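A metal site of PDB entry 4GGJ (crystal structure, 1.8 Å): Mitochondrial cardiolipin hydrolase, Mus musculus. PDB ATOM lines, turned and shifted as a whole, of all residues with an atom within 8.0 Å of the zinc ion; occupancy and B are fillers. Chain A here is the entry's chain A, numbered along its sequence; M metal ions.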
ATOM      1  N   THR A  19      -3.835 -18.189  26.715  1.00  0.00           N
ATOM      2  CA  THR A  19      -3.270 -19.275  25.905  1.00  0.00           C
ATOM      3  C   THR A  19      -4.267 -19.618  24.817  1.00  0.00           C
ATOM      4  O   THR A  19      -5.450 -19.275  24.923  1.00  0.00           O
ATOM      5  CB  THR A  19      -2.976 -20.519  26.771  1.00  0.00           C
ATOM      6  OG1 THR A  19      -4.184 -21.031  27.332  1.00  0.00           O
ATOM      7  CG2 THR A  19      -1.985 -20.178  27.888  1.00  0.00           C
ATOM      8  N   CYS A  20      -3.784 -20.314  23.802  1.00  0.00           N
ATOM      9  CA  CYS A  20      -4.587 -20.717  22.662  1.00  0.00           C
ATOM     10  C   CYS A  20      -5.541 -21.884  23.003  1.00  0.00           C
ATOM     11  O   CYS A  20      -5.117 -22.867  23.625  1.00  0.00           O
ATOM     12  CB  CYS A  20      -3.663 -21.105  21.506  1.00  0.00           C
ATOM     13  SG  CYS A  20      -4.529 -21.651  20.060  1.00  0.00           S
ATOM     14  N   THR A  21      -6.807 -21.763  22.592  1.00  0.00           N
ATOM     15  CA  THR A  21      -7.803 -22.803  22.841  1.00  0.00           C
ATOM     16  C   THR A  21      -8.511 -23.237  21.551  1.00  0.00           C
ATOM     17  O   THR A  21      -9.555 -23.876  21.596  1.00  0.00           O
ATOM     18  CB  THR A  21      -8.857 -22.310  23.853  1.00  0.00           C
ATOM     19  OG1 THR A  21      -9.539 -21.162  23.340  1.00  0.00           O
ATOM     20  CG2 THR A  21      -8.179 -21.937  25.203  1.00  0.00           C
ATOM     21  N   GLU A  22      -7.913 -22.922  20.403  1.00  0.00           N
ATOM     22  CA  GLU A  22      -8.545 -23.153  19.105  1.00  0.00           C
ATOM     23  C   GLU A  22      -8.801 -24.634  18.856  1.00  0.00           C
ATOM     24  O   GLU A  22      -9.887 -25.009  18.410  1.00  0.00           O
ATOM     25  CB  GLU A  22      -7.695 -22.582  17.973  1.00  0.00           C
ATOM     26  CG  GLU A  22      -7.507 -21.065  18.016  1.00  0.00           C
ATOM     27  CD  GLU A  22      -8.802 -20.294  17.875  1.00  0.00           C
ATOM     28  OE1 GLU A  22      -9.342 -20.227  16.748  1.00  0.00           O
ATOM     29  OE2 GLU A  22      -9.263 -19.749  18.906  1.00  0.00           O
ATOM     30  N   ALA A  23      -7.806 -25.471  19.134  1.00  0.00           N
ATOM     31  CA  ALA A  23      -7.935 -26.914  18.894  1.00  0.00           C
ATOM     32  C   ALA A  23      -8.919 -27.526  19.871  1.00  0.00           C
ATOM     33  O   ALA A  23      -9.790 -28.323  19.487  1.00  0.00           O
ATOM     34  CB  ALA A  23      -6.573 -27.591  18.987  1.00  0.00           C
ATOM     35  N   CYS A  37      -1.599 -25.138  14.914  1.00  0.00           N
ATOM     36  CA  CYS A  37      -2.131 -23.780  14.913  1.00  0.00           C
ATOM     37  C   CYS A  37      -1.005 -22.782  14.662  1.00  0.00           C
ATOM     38  O   CYS A  37       0.074 -22.922  15.238  1.00  0.00           O
ATOM     39  CB  CYS A  37      -2.814 -23.486  16.246  1.00  0.00           C
ATOM     40  SG  CYS A  37      -3.466 -21.800  16.419  1.00  0.00           S
ATOM     41  N   PRO A  38      -1.257 -21.781  13.797  1.00  0.00           N
ATOM     42  CA  PRO A  38      -0.252 -20.760  13.478  1.00  0.00           C
ATOM     43  C   PRO A  38      -0.356 -19.472  14.303  1.00  0.00           C
ATOM     44  O   PRO A  38       0.266 -18.477  13.946  1.00  0.00           O
ATOM     45  CB  PRO A  38      -0.577 -20.441  12.013  1.00  0.00           C
ATOM     46  CG  PRO A  38      -2.075 -20.530  11.964  1.00  0.00           C
ATOM     47  CD  PRO A  38      -2.435 -21.645  12.927  1.00  0.00           C
ATOM     48  N   CYS A  39      -1.139 -19.465  15.388  1.00  0.00           N
ATOM     49  CA  CYS A  39      -1.348 -18.237  16.140  1.00  0.00           C
ATOM     50  C   CYS A  39      -0.132 -17.906  17.011  1.00  0.00           C
ATOM     51  O   CYS A  39       0.788 -18.724  17.159  1.00  0.00           O
ATOM     52  CB  CYS A  39      -2.624 -18.320  16.981  1.00  0.00           C
ATOM     53  SG  CYS A  39      -2.424 -19.081  18.593  1.00  0.00           S
ATOM     54  N   SER A  40      -0.140 -16.711  17.593  1.00  0.00           N
ATOM     55  CA  SER A  40       0.980 -16.186  18.368  1.00  0.00           C
ATOM     56  C   SER A  40       0.885 -16.448  19.874  1.00  0.00           C
ATOM     57  O   SER A  40       1.821 -16.126  20.605  1.00  0.00           O
ATOM     58  CB  SER A  40       1.111 -14.674  18.144  1.00  0.00           C
ATOM     59  OG  SER A  40       1.302 -14.384  16.771  1.00  0.00           O
ATOM     60  N   LEU A  41      -0.221 -17.034  20.340  1.00  0.00           N
ATOM     61  CA  LEU A  41      -0.377 -17.289  21.763  1.00  0.00           C
ATOM     62  C   LEU A  41       0.359 -18.569  22.201  1.00  0.00           C
ATOM     63  O   LEU A  41       0.620 -19.450  21.380  1.00  0.00           O
ATOM     64  CB  LEU A  41      -1.858 -17.411  22.149  1.00  0.00           C
ATOM     65  CG  LEU A  41      -2.750 -16.167  22.031  1.00  0.00           C
ATOM     66  CD1 LEU A  41      -4.196 -16.521  22.341  1.00  0.00           C
ATOM     67  CD2 LEU A  41      -2.260 -15.059  22.932  1.00  0.00           C
ATOM     68  N   PRO A  42       0.687 -18.654  23.494  1.00  0.00           N
ATOM     69  CA  PRO A  42       1.264 -19.891  24.035  1.00  0.00           C
ATOM     70  C   PRO A  42       0.322 -21.081  23.842  1.00  0.00           C
ATOM     71  O   PRO A  42      -0.896 -20.958  24.031  1.00  0.00           O
ATOM     72  CB  PRO A  42       1.431 -19.590  25.532  1.00  0.00           C
ATOM     73  CG  PRO A  42       1.467 -18.115  25.631  1.00  0.00           C
ATOM     74  CD  PRO A  42       0.646 -17.580  24.507  1.00  0.00           C
ATOM     75  N   HIS A  43       0.897 -22.215  23.478  1.00  0.00           N
ATOM     76  CA  HIS A  43       0.120 -23.440  23.312  1.00  0.00           C
ATOM     77  C   HIS A  43       0.386 -24.368  24.483  1.00  0.00           C
ATOM     78  O   HIS A  43       1.020 -25.413  24.354  1.00  0.00           O
ATOM     79  CB  HIS A  43       0.428 -24.079  21.963  1.00  0.00           C
ATOM     80  CG  HIS A  43      -0.118 -23.295  20.809  1.00  0.00           C
ATOM     81  ND1 HIS A  43       0.552 -22.242  20.245  1.00  0.00           N
ATOM     82  CD2 HIS A  43      -1.293 -23.396  20.147  1.00  0.00           C
ATOM     83  CE1 HIS A  43      -0.177 -21.739  19.262  1.00  0.00           C
ATOM     84  NE2 HIS A  43      -1.300 -22.421  19.185  1.00  0.00           N
HETATM   85 ZN    ZN M   1      -3.020 -21.176  18.497  1.00  0.00          ZN
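SG of Cys 20 sits close to N of Glu 22 (3.6 Å).
The backbone NH of Leu 41 lies close to the side-chain sulfur of Cys 39, 3.5 Å away.
O of Leu 41 is in hydrogen-bond range of ND1 of His 43 (3.0 Å).
N of Cys 20 lies within hydrogen-bond range of O of Pro 42 (3.0 Å).
The zinc ion is bound by SG of Cys 39, SG of Cys 37, SG of Cys 20 and NE2 of His 43.
Four residues have an atom within 4 Å of the zinc ion: Cys 20, Cys 37, Cys 39 and His 43.
Along chain A the residues within 4 Å of the zinc ion span positions 20 to 43.
The nearest printed residue that does not touch the zinc ion is Glu 22 (4.5 Å).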
